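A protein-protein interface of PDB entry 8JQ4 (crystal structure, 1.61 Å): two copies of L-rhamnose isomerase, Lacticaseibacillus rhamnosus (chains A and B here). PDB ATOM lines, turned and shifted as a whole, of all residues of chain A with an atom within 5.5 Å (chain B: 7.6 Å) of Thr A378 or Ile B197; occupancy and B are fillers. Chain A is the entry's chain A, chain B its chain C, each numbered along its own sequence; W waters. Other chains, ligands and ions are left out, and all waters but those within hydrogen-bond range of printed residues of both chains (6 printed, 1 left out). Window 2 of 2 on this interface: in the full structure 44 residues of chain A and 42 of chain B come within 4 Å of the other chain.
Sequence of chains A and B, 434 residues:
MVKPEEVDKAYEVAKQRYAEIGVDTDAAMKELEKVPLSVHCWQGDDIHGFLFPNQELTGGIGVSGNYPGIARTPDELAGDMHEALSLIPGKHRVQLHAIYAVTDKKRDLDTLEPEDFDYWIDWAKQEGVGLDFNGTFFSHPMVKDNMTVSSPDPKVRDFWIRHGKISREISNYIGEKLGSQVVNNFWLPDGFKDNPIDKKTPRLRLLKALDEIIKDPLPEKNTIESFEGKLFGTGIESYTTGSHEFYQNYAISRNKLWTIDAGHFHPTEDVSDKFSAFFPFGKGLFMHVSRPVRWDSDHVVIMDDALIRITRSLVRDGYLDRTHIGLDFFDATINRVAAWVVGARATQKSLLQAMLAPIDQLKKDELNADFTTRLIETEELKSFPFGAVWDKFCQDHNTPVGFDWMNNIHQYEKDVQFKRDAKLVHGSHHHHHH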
ATOM      1  N   ARG A 316      -5.363   4.368   3.128  1.00  0.00           N
ATOM      2  CA  ARG A 316      -5.869   3.086   2.567  1.00  0.00           C
ATOM      3  C   ARG A 316      -4.777   2.013   2.654  1.00  0.00           C
ATOM      4  O   ARG A 316      -5.127   0.845   2.881  1.00  0.00           O
ATOM      5  CB  ARG A 316      -6.336   3.258   1.120  1.00  0.00           C
ATOM      6  CG  ARG A 316      -7.652   4.008   0.987  1.00  0.00           C
ATOM      7  CD  ARG A 316      -7.888   4.459  -0.440  1.00  0.00           C
ATOM      8  NE  ARG A 316      -9.207   5.049  -0.602  1.00  0.00           N
ATOM      9  CZ  ARG A 316      -9.719   5.435  -1.760  1.00  0.00           C
ATOM     10  NH1 ARG A 316      -9.024   5.298  -2.876  1.00  0.00           N
ATOM     11  NH2 ARG A 316     -10.937   5.939  -1.798  1.00  0.00           N
ATOM     12  N   ASP A 317      -3.514   2.384   2.437  1.00  0.00           N
ATOM     13  CA  ASP A 317      -2.402   1.404   2.293  1.00  0.00           C
ATOM     14  C   ASP A 317      -1.579   1.370   3.586  1.00  0.00           C
ATOM     15  O   ASP A 317      -0.570   0.634   3.617  1.00  0.00           O
ATOM     16  CB  ASP A 317      -1.567   1.709   1.047  1.00  0.00           C
ATOM     17  CG  ASP A 317      -2.273   1.359  -0.255  1.00  0.00           C
ATOM     18  OD1 ASP A 317      -3.035   0.372  -0.266  1.00  0.00           O
ATOM     19  OD2 ASP A 317      -2.036   2.057  -1.255  1.00  0.00           O
ATOM     20  N   ILE A 359     -12.934   0.529   4.085  1.00  0.00           N
ATOM     21  CA  ILE A 359     -11.725   0.249   3.259  1.00  0.00           C
ATOM     22  C   ILE A 359     -11.567  -1.269   3.092  1.00  0.00           C
ATOM     23  O   ILE A 359     -11.345  -1.713   1.948  1.00  0.00           O
ATOM     24  CB  ILE A 359     -10.476   0.926   3.855  1.00  0.00           C
ATOM     25  CG1 ILE A 359     -10.621   2.451   3.854  1.00  0.00           C
ATOM     26  CG2 ILE A 359      -9.225   0.487   3.117  1.00  0.00           C
ATOM     27  CD1 ILE A 359      -9.526   3.173   4.604  1.00  0.00           C
ATOM     28  N   LEU A 362     -14.156  -2.468   0.560  1.00  0.00           N
ATOM     29  CA  LEU A 362     -13.825  -1.920  -0.780  1.00  0.00           C
ATOM     30  C   LEU A 362     -12.638  -2.691  -1.365  1.00  0.00           C
ATOM     31  O   LEU A 362     -12.651  -2.968  -2.585  1.00  0.00           O
ATOM     32  CB  LEU A 362     -13.531  -0.423  -0.658  1.00  0.00           C
ATOM     33  CG  LEU A 362     -14.765   0.473  -0.612  1.00  0.00           C
ATOM     34  CD1 LEU A 362     -14.390   1.873  -0.161  1.00  0.00           C
ATOM     35  CD2 LEU A 362     -15.458   0.506  -1.966  1.00  0.00           C
ATOM     36  N   LYS A 363     -11.652  -3.035  -0.533  1.00  0.00           N
ATOM     37  CA  LYS A 363     -10.471  -3.823  -0.973  1.00  0.00           C
ATOM     38  C   LYS A 363     -10.934  -5.190  -1.480  1.00  0.00           C
ATOM     39  O   LYS A 363     -10.456  -5.597  -2.546  1.00  0.00           O
ATOM     40  CB  LYS A 363      -9.444  -3.957   0.153  1.00  0.00           C
ATOM     41  CG  LYS A 363      -8.591  -2.720   0.369  1.00  0.00           C
ATOM     42  CD  LYS A 363      -7.617  -2.882   1.497  1.00  0.00           C
ATOM     43  CE  LYS A 363      -6.599  -1.768   1.567  1.00  0.00           C
ATOM     44  NZ  LYS A 363      -5.744  -1.914   2.766  1.00  0.00           N
ATOM     45  N   GLU A 366     -12.706  -4.890  -4.803  1.00  0.00           N
ATOM     46  CA  GLU A 366     -11.676  -4.615  -5.836  1.00  0.00           C
ATOM     47  C   GLU A 366     -10.925  -5.910  -6.186  1.00  0.00           C
ATOM     48  O   GLU A 366     -10.678  -6.141  -7.386  1.00  0.00           O
ATOM     49  CB  GLU A 366     -10.736  -3.532  -5.318  1.00  0.00           C
ATOM     50  CG  GLU A 366      -9.576  -3.238  -6.240  1.00  0.00           C
ATOM     51  CD  GLU A 366      -8.811  -1.999  -5.818  1.00  0.00           C
ATOM     52  OE1 GLU A 366      -7.936  -2.121  -4.936  1.00  0.00           O
ATOM     53  OE2 GLU A 366      -9.168  -0.903  -6.294  1.00  0.00           O
ATOM     54  N   THR A 373     -19.299  -1.589  -8.083  1.00  0.00           N
ATOM     55  CA  THR A 373     -19.501  -1.263  -6.647  1.00  0.00           C
ATOM     56  C   THR A 373     -18.439  -0.249  -6.205  1.00  0.00           C
ATOM     57  O   THR A 373     -18.797   0.709  -5.504  1.00  0.00           O
ATOM     58  CB  THR A 373     -19.482  -2.519  -5.768  1.00  0.00           C
ATOM     59  OG1 THR A 373     -20.568  -3.350  -6.180  1.00  0.00           O
ATOM     60  CG2 THR A 373     -19.600  -2.199  -4.295  1.00  0.00           C
ATOM     61  N   ARG A 374     -17.178  -0.440  -6.598  1.00  0.00           N
ATOM     62  CA  ARG A 374     -16.079   0.466  -6.173  1.00  0.00           C
ATOM     63  C   ARG A 374     -16.399   1.894  -6.634  1.00  0.00           C
ATOM     64  O   ARG A 374     -16.272   2.822  -5.814  1.00  0.00           O
ATOM     65  CB  ARG A 374     -14.722   0.023  -6.721  1.00  0.00           C
ATOM     66  CG  ARG A 374     -13.561   0.860  -6.199  1.00  0.00           C
ATOM     67  CD  ARG A 374     -12.241   0.516  -6.866  1.00  0.00           C
ATOM     68  NE  ARG A 374     -12.309   0.733  -8.305  1.00  0.00           N
ATOM     69  CZ  ARG A 374     -11.502   0.168  -9.194  1.00  0.00           C
ATOM     70  NH1 ARG A 374     -10.548  -0.660  -8.801  1.00  0.00           N
ATOM     71  NH2 ARG A 374     -11.657   0.425 -10.480  1.00  0.00           N
ATOM     72  N   LEU A 375     -16.777   2.072  -7.902  1.00  0.00           N
ATOM     73  CA  LEU A 375     -17.051   3.417  -8.475  1.00  0.00           C
ATOM     74  C   LEU A 375     -18.240   4.039  -7.740  1.00  0.00           C
ATOM     75  O   LEU A 375     -18.137   5.218  -7.339  1.00  0.00           O
ATOM     76  CB  LEU A 375     -17.340   3.318  -9.974  1.00  0.00           C
ATOM     77  CG  LEU A 375     -17.620   4.655 -10.659  1.00  0.00           C
ATOM     78  CD1 LEU A 375     -16.419   5.582 -10.552  1.00  0.00           C
ATOM     79  CD2 LEU A 375     -18.021   4.454 -12.116  1.00  0.00           C
ATOM     80  N   ILE A 376     -19.348   3.304  -7.623  1.00  0.00           N
ATOM     81  CA  ILE A 376     -20.597   3.846  -7.015  1.00  0.00           C
ATOM     82  C   ILE A 376     -20.283   4.287  -5.583  1.00  0.00           C
ATOM     83  O   ILE A 376     -20.648   5.414  -5.216  1.00  0.00           O
ATOM     84  CB  ILE A 376     -21.758   2.838  -7.048  1.00  0.00           C
ATOM     85  CG1 ILE A 376     -22.175   2.486  -8.479  1.00  0.00           C
ATOM     86  CG2 ILE A 376     -22.926   3.382  -6.239  1.00  0.00           C
ATOM     87  CD1 ILE A 376     -23.202   1.379  -8.560  1.00  0.00           C
ATOM     88  N   GLU A 377     -19.635   3.429  -4.794  1.00  0.00           N
ATOM     89  CA  GLU A 377     -19.444   3.691  -3.347  1.00  0.00           C
ATOM     90  C   GLU A 377     -18.466   4.857  -3.165  1.00  0.00           C
ATOM     91  O   GLU A 377     -18.756   5.737  -2.351  1.00  0.00           O
ATOM     92  CB  GLU A 377     -18.989   2.425  -2.622  1.00  0.00           C
ATOM     93  CG  GLU A 377     -20.081   1.376  -2.543  1.00  0.00           C
ATOM     94  CD  GLU A 377     -19.792   0.252  -1.565  1.00  0.00           C
ATOM     95  OE1 GLU A 377     -18.734   0.305  -0.908  1.00  0.00           O
ATOM     96  OE2 GLU A 377     -20.623  -0.669  -1.463  1.00  0.00           O
ATOM     97  N   THR A 378     -17.319   4.851  -3.850  1.00  0.00           N
ATOM     98  CA  THR A 378     -16.303   5.921  -3.676  1.00  0.00           C
ATOM     99  C   THR A 378     -16.959   7.264  -4.018  1.00  0.00           C
ATOM    100  O   THR A 378     -16.723   8.242  -3.287  1.00  0.00           O
ATOM    101  CB  THR A 378     -15.015   5.636  -4.460  1.00  0.00           C
ATOM    102  OG1 THR A 378     -15.310   5.367  -5.830  1.00  0.00           O
ATOM    103  CG2 THR A 378     -14.245   4.468  -3.880  1.00  0.00           C
ATOM    104  N   GLU A 379     -17.833   7.293  -5.025  1.00  0.00           N
ATOM    105  CA  GLU A 379     -18.522   8.541  -5.443  1.00  0.00           C
ATOM    106  C   GLU A 379     -19.573   8.926  -4.392  1.00  0.00           C
ATOM    107  O   GLU A 379     -19.641  10.121  -4.045  1.00  0.00           O
ATOM    108  CB  GLU A 379     -19.095   8.378  -6.849  1.00  0.00           C
ATOM    109  CG  GLU A 379     -18.028   8.509  -7.916  1.00  0.00           C
ATOM    110  CD  GLU A 379     -17.155   9.738  -7.734  1.00  0.00           C
ATOM    111  OE1 GLU A 379     -17.717  10.861  -7.732  1.00  0.00           O
ATOM    112  OE2 GLU A 379     -15.923   9.574  -7.550  1.00  0.00           O
ATOM    113  N   GLU A 380     -20.322   7.965  -3.849  1.00  0.00           N
ATOM    114  CA  GLU A 380     -21.357   8.265  -2.823  1.00  0.00           C
ATOM    115  C   GLU A 380     -20.667   8.825  -1.571  1.00  0.00           C
ATOM    116  O   GLU A 380     -21.200   9.757  -0.958  1.00  0.00           O
ATOM    117  CB  GLU A 380     -22.215   7.039  -2.517  1.00  0.00           C
ATOM    118  CG  GLU A 380     -23.153   6.654  -3.647  1.00  0.00           C
ATOM    119  CD  GLU A 380     -24.072   7.762  -4.139  1.00  0.00           C
ATOM    120  OE1 GLU A 380     -24.481   8.601  -3.312  1.00  0.00           O
ATOM    121  OE2 GLU A 380     -24.370   7.786  -5.352  1.00  0.00           O
ATOM    122  N   LEU A 381     -19.500   8.296  -1.201  1.00  0.00           N
ATOM    123  CA  LEU A 381     -18.810   8.708   0.047  1.00  0.00           C
ATOM    124  C   LEU A 381     -18.396  10.182  -0.022  1.00  0.00           C
ATOM    125  O   LEU A 381     -18.296  10.814   1.044  1.00  0.00           O
ATOM    126  CB  LEU A 381     -17.612   7.783   0.270  1.00  0.00           C
ATOM    127  CG  LEU A 381     -18.006   6.382   0.726  1.00  0.00           C
ATOM    128  CD1 LEU A 381     -16.834   5.427   0.626  1.00  0.00           C
ATOM    129  CD2 LEU A 381     -18.567   6.417   2.138  1.00  0.00           C
ATOM    130  N   LYS A 382     -18.227  10.741  -1.221  1.00  0.00           N
ATOM    131  CA  LYS A 382     -17.814  12.160  -1.371  1.00  0.00           C
ATOM    132  C   LYS A 382     -18.938  13.086  -0.885  1.00  0.00           C
ATOM    133  O   LYS A 382     -18.626  14.246  -0.561  1.00  0.00           O
ATOM    134  CB  LYS A 382     -17.419  12.454  -2.818  1.00  0.00           C
ATOM    135  CG  LYS A 382     -16.222  11.657  -3.313  1.00  0.00           C
ATOM    136  CD  LYS A 382     -15.788  12.038  -4.700  1.00  0.00           C
ATOM    137  CE  LYS A 382     -14.464  11.422  -5.091  1.00  0.00           C
ATOM    138  NZ  LYS A 382     -14.200  11.573  -6.539  1.00  0.00           N
ATOM    139  N   PHE B 192      -5.013  -0.775 -13.404  1.00  0.00           N
ATOM    140  CA  PHE B 192      -6.468  -0.510 -13.312  1.00  0.00           C
ATOM    141  C   PHE B 192      -6.870   0.564 -14.318  1.00  0.00           C
ATOM    142  O   PHE B 192      -6.145   1.568 -14.483  1.00  0.00           O
ATOM    143  CB  PHE B 192      -6.858  -0.064 -11.905  1.00  0.00           C
ATOM    144  CG  PHE B 192      -6.824  -1.154 -10.866  1.00  0.00           C
ATOM    145  CD1 PHE B 192      -7.822  -2.113 -10.811  1.00  0.00           C
ATOM    146  CD2 PHE B 192      -5.816  -1.193  -9.920  1.00  0.00           C
ATOM    147  CE1 PHE B 192      -7.819  -3.080  -9.822  1.00  0.00           C
ATOM    148  CE2 PHE B 192      -5.806  -2.170  -8.938  1.00  0.00           C
ATOM    149  CZ  PHE B 192      -6.810  -3.107  -8.887  1.00  0.00           C
ATOM    150  N   ASP B 194      -9.668   2.356 -13.680  1.00  0.00           N
ATOM    151  CA  ASP B 194     -10.227   3.416 -12.802  1.00  0.00           C
ATOM    152  C   ASP B 194      -9.466   3.409 -11.472  1.00  0.00           C
ATOM    153  O   ASP B 194      -8.553   2.581 -11.315  1.00  0.00           O
ATOM    154  CB  ASP B 194     -11.742   3.265 -12.641  1.00  0.00           C
ATOM    155  CG  ASP B 194     -12.473   4.597 -12.672  1.00  0.00           C
ATOM    156  OD1 ASP B 194     -11.982   5.545 -12.034  1.00  0.00           O
ATOM    157  OD2 ASP B 194     -13.503   4.687 -13.374  1.00  0.00           O
ATOM    158  N   ASN B 195      -9.786   4.349 -10.582  1.00  0.00           N
ATOM    159  CA  ASN B 195      -8.986   4.655  -9.364  1.00  0.00           C
ATOM    160  C   ASN B 195      -9.000   3.454  -8.424  1.00  0.00           C
ATOM    161  O   ASN B 195     -10.058   2.990  -8.005  1.00  0.00           O
ATOM    162  CB  ASN B 195      -9.502   5.914  -8.666  1.00  0.00           C
ATOM    163  CG  ASN B 195      -9.255   7.163  -9.483  1.00  0.00           C
ATOM    164  OD1 ASN B 195      -8.149   7.377  -9.975  1.00  0.00           O
ATOM    165  ND2 ASN B 195     -10.289   7.968  -9.677  1.00  0.00           N
ATOM    166  N   PRO B 196      -7.820   2.915  -8.046  1.00  0.00           N
ATOM    167  CA  PRO B 196      -7.768   1.789  -7.117  1.00  0.00           C
ATOM    168  C   PRO B 196      -7.863   2.190  -5.639  1.00  0.00           C
ATOM    169  O   PRO B 196      -7.504   3.302  -5.288  1.00  0.00           O
ATOM    170  CB  PRO B 196      -6.393   1.185  -7.427  1.00  0.00           C
ATOM    171  CG  PRO B 196      -5.553   2.381  -7.789  1.00  0.00           C
ATOM    172  CD  PRO B 196      -6.497   3.270  -8.580  1.00  0.00           C
ATOM    173  N   ILE B 197      -8.315   1.250  -4.809  1.00  0.00           N
ATOM    174  CA  ILE B 197      -8.346   1.369  -3.324  1.00  0.00           C
ATOM    175  C   ILE B 197      -6.967   0.993  -2.774  1.00  0.00           C
ATOM    176  O   ILE B 197      -6.442   1.742  -1.930  1.00  0.00           O
ATOM    177  CB  ILE B 197      -9.460   0.481  -2.739  1.00  0.00           C
ATOM    178  CG1 ILE B 197     -10.816   0.770  -3.389  1.00  0.00           C
ATOM    179  CG2 ILE B 197      -9.517   0.624  -1.228  1.00  0.00           C
ATOM    180  CD1 ILE B 197     -11.258   2.207  -3.262  1.00  0.00           C
ATOM    181  N   ASP B 198      -6.408  -0.121  -3.257  1.00  0.00           N
ATOM    182  CA  ASP B 198      -5.161  -0.729  -2.716  1.00  0.00           C
ATOM    183  C   ASP B 198      -4.055  -0.644  -3.774  1.00  0.00           C
ATOM    184  O   ASP B 198      -4.103  -1.401  -4.762  1.00  0.00           O
ATOM    185  CB  ASP B 198      -5.412  -2.164  -2.249  1.00  0.00           C
ATOM    186  CG  ASP B 198      -4.209  -2.784  -1.565  1.00  0.00           C
ATOM    187  OD1 ASP B 198      -3.086  -2.280  -1.789  1.00  0.00           O
ATOM    188  OD2 ASP B 198      -4.411  -3.749  -0.802  1.00  0.00           O
ATOM    189  N   LYS B 199      -3.122   0.291  -3.592  1.00  0.00           N
ATOM    190  CA  LYS B 199      -1.973   0.507  -4.508  1.00  0.00           C
ATOM    191  C   LYS B 199      -0.791  -0.343  -4.038  1.00  0.00           C
ATOM    192  O   LYS B 199       0.132  -0.569  -4.842  1.00  0.00           O
ATOM    193  CB  LYS B 199      -1.577   1.982  -4.515  1.00  0.00           C
ATOM    194  CG  LYS B 199      -2.637   2.922  -5.077  1.00  0.00           C
ATOM    195  CD  LYS B 199      -2.153   4.343  -5.120  1.00  0.00           C
ATOM    196  CE  LYS B 199      -3.189   5.300  -5.675  1.00  0.00           C
ATOM    197  NZ  LYS B 199      -2.648   6.677  -5.737  1.00  0.00           N
ATOM    198  N   LYS B 200      -0.793  -0.707  -2.755  1.00  0.00           N
ATOM    199  CA  LYS B 200       0.334  -1.406  -2.084  1.00  0.00           C
ATOM    200  C   LYS B 200       0.373  -2.872  -2.527  1.00  0.00           C
ATOM    201  O   LYS B 200       1.449  -3.333  -2.959  1.00  0.00           O
ATOM    202  CB  LYS B 200       0.189  -1.312  -0.565  1.00  0.00           C
ATOM    203  CG  LYS B 200       1.175  -2.170   0.215  1.00  0.00           C
ATOM    204  CD  LYS B 200       1.099  -1.954   1.703  1.00  0.00           C
ATOM    205  CE  LYS B 200      -0.046  -2.707   2.339  1.00  0.00           C
ATOM    206  NZ  LYS B 200      -0.167  -2.393   3.782  1.00  0.00           N
ATOM    207  N   PRO B 202      -0.879  -4.849  -5.011  1.00  0.00           N
ATOM    208  CA  PRO B 202      -0.476  -5.256  -6.357  1.00  0.00           C
ATOM    209  C   PRO B 202       1.048  -5.200  -6.553  1.00  0.00           C
ATOM    210  O   PRO B 202       1.601  -6.071  -7.216  1.00  0.00           O
ATOM    211  CB  PRO B 202      -1.185  -4.246  -7.268  1.00  0.00           C
ATOM    212  CG  PRO B 202      -2.391  -3.834  -6.461  1.00  0.00           C
ATOM    213  CD  PRO B 202      -1.885  -3.768  -5.035  1.00  0.00           C
HETATM  214  O   HOH W   1      -3.297  -1.756   1.391  1.00  0.00           O
HETATM  215  O   HOH W   2      -5.574  -3.581  -5.547  1.00  0.00           O
HETATM  216  O   HOH W   3      -5.975   5.053  -3.278  1.00  0.00           O
HETATM  217  O   HOH W   4       1.501  -0.588   5.162  1.00  0.00           O
HETATM  218  O   HOH W   5      -4.413   3.573  -1.794  1.00  0.00           O
HETATM  219  O   HOH W   6     -10.708  -0.385 -13.008  1.00  0.00           O
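The side-chain carboxylate (OD2) of Asp A317 lies within hydrogen-bond range of the backbone NH (N) of Lys B199 (3.1 Å). The side-chain carboxylate (OD1) of Asp A317 sits close to the side-chain carboxylate (OD1) of Asp B198 (3.1 Å). The backbone carbonyl oxygen (O) of Asn B195 lies within hydrogen-bond range of the guanidinium group (NE) of Arg A374 (3.2 Å). The side-chain carboxylate of Glu A366 sits at hydrogen-bond distance from the backbone NH of Asp B198, at 3.0 Å. The side-chain carboxylate (OE2) of Glu A366 sits at hydrogen-bond distance from the backbone NH (N) of Ile B197 (2.8 Å). O of Pro B196 lies within hydrogen-bond range of NH1 of Arg A316 (3.5 Å). NZ of Lys B200 lies within hydrogen-bond range of O of Asp A317.
Ile B197 touches Arg A316. Lys A363 touches Ile B197 (CG to CG2, 3.8 Å). Asp B198 touches Lys A363 (OD2 to CE, 3.8 Å). Phe B192 touches Glu A366 (CZ to CD, 3.8 Å). Glu A366 touches Pro B196. Arg A374 touches Phe B192 (NH1 to CD1, 3.7 Å). NH2 of Arg A374 touches CB of Asp B194, at 3.6 Å. Arg A374 touches Ile B197. Thr A378 touches Ile B197.
Along chain A the printed residues that touch a printed residue of chain B span positions 316 to 378. Of the 9 printed residues of chain B, 8 touch a printed residue of chain A. Printed residues of chain B that touch a printed residue of chain A: Phe B192, Asp B194, Asn B195, Pro B196, Ile B197, Asp B198, Lys B199 and Lys B200. Among the printed residues, 16 pairs touch across the chains.
No position is printed for both chains.
Water W1 lies within hydrogen-bond range of OD1 of Asp A317 (2.7 Å), NZ of Lys A363 (2.8 Å) and OD2 of Asp B198 (3.2 Å). Water W5 bridges the backbone carbonyl oxygen of Ile B197 (2.7 Å) and the side-chain carboxylate of Asp A317 (2.9 Å). Water W2 lies within hydrogen-bond range of the backbone carbonyl oxygen (O) of Asp B198 (2.7 Å) and the side-chain carboxylate (OE1) of Glu A366 (2.8 Å). Water W4 lies within hydrogen-bond range of NZ of Lys B200 (2.8 Å) and O of Asp A317 (2.9 Å). Water W6 bridges the guanidinium group of Arg A374 (2.8 Å) and the backbone NH of Asp B194 (3.0 Å). Water W3 lies within hydrogen-bond range of the backbone carbonyl oxygen of Pro B196 (3.1 Å) and the guanidinium group of Arg A316 (3.1 Å).
Of the printed residues of chain B, Arg A316 touches Pro B196 and Ile B197. Printed residues of chain B within 4 Å of Lys A363: Ile B197 (3.8 Å) and Asp B198 (3.8 Å). Leu A375 touches none of the printed residues of chain B. Thr A378 touches just one residue of chain B: Ile B197. Glu A379 touches none of the printed residues of chain B. Printed residues of chain A within 4 Å of Phe B192: Glu A366 (3.8 Å) and Arg A374 (3.7 Å). Printed residues of chain A within 4 Å of Asn B195: Arg A374 (3.2 Å). Of chain A, only Arg A316 (3.4 Å), Lys A363 (3.8 Å), Glu A366 (2.8 Å), Arg A374 (3.8 Å) and Thr A378 (3.8 Å) come within 4 Å of Ile B197. Printed residues of chain A within 4 Å of Lys B199: Asp A317. The nearest residue of chain B that does not touch Thr A378 is Asn B195 (6.1 Å).
The side-chain carboxylate of Glu A366 lies within salt-bridge range of the guanidinium group of Arg A374. O of Leu A375 lies within hydrogen-bond range of OG1 of Thr A378. N of Lys B200 is in hydrogen-bond range of OD1 of Asp B198, at 2.9 Å. The side-chain amino group of Lys A363 is in hydrogen-bond range of the backbone carbonyl oxygen of Arg A316. The side-chain hydroxyl (OG1) of Thr A378 sits at hydrogen-bond distance from the backbone carbonyl oxygen (O) of Arg A374, at 2.7 Å.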
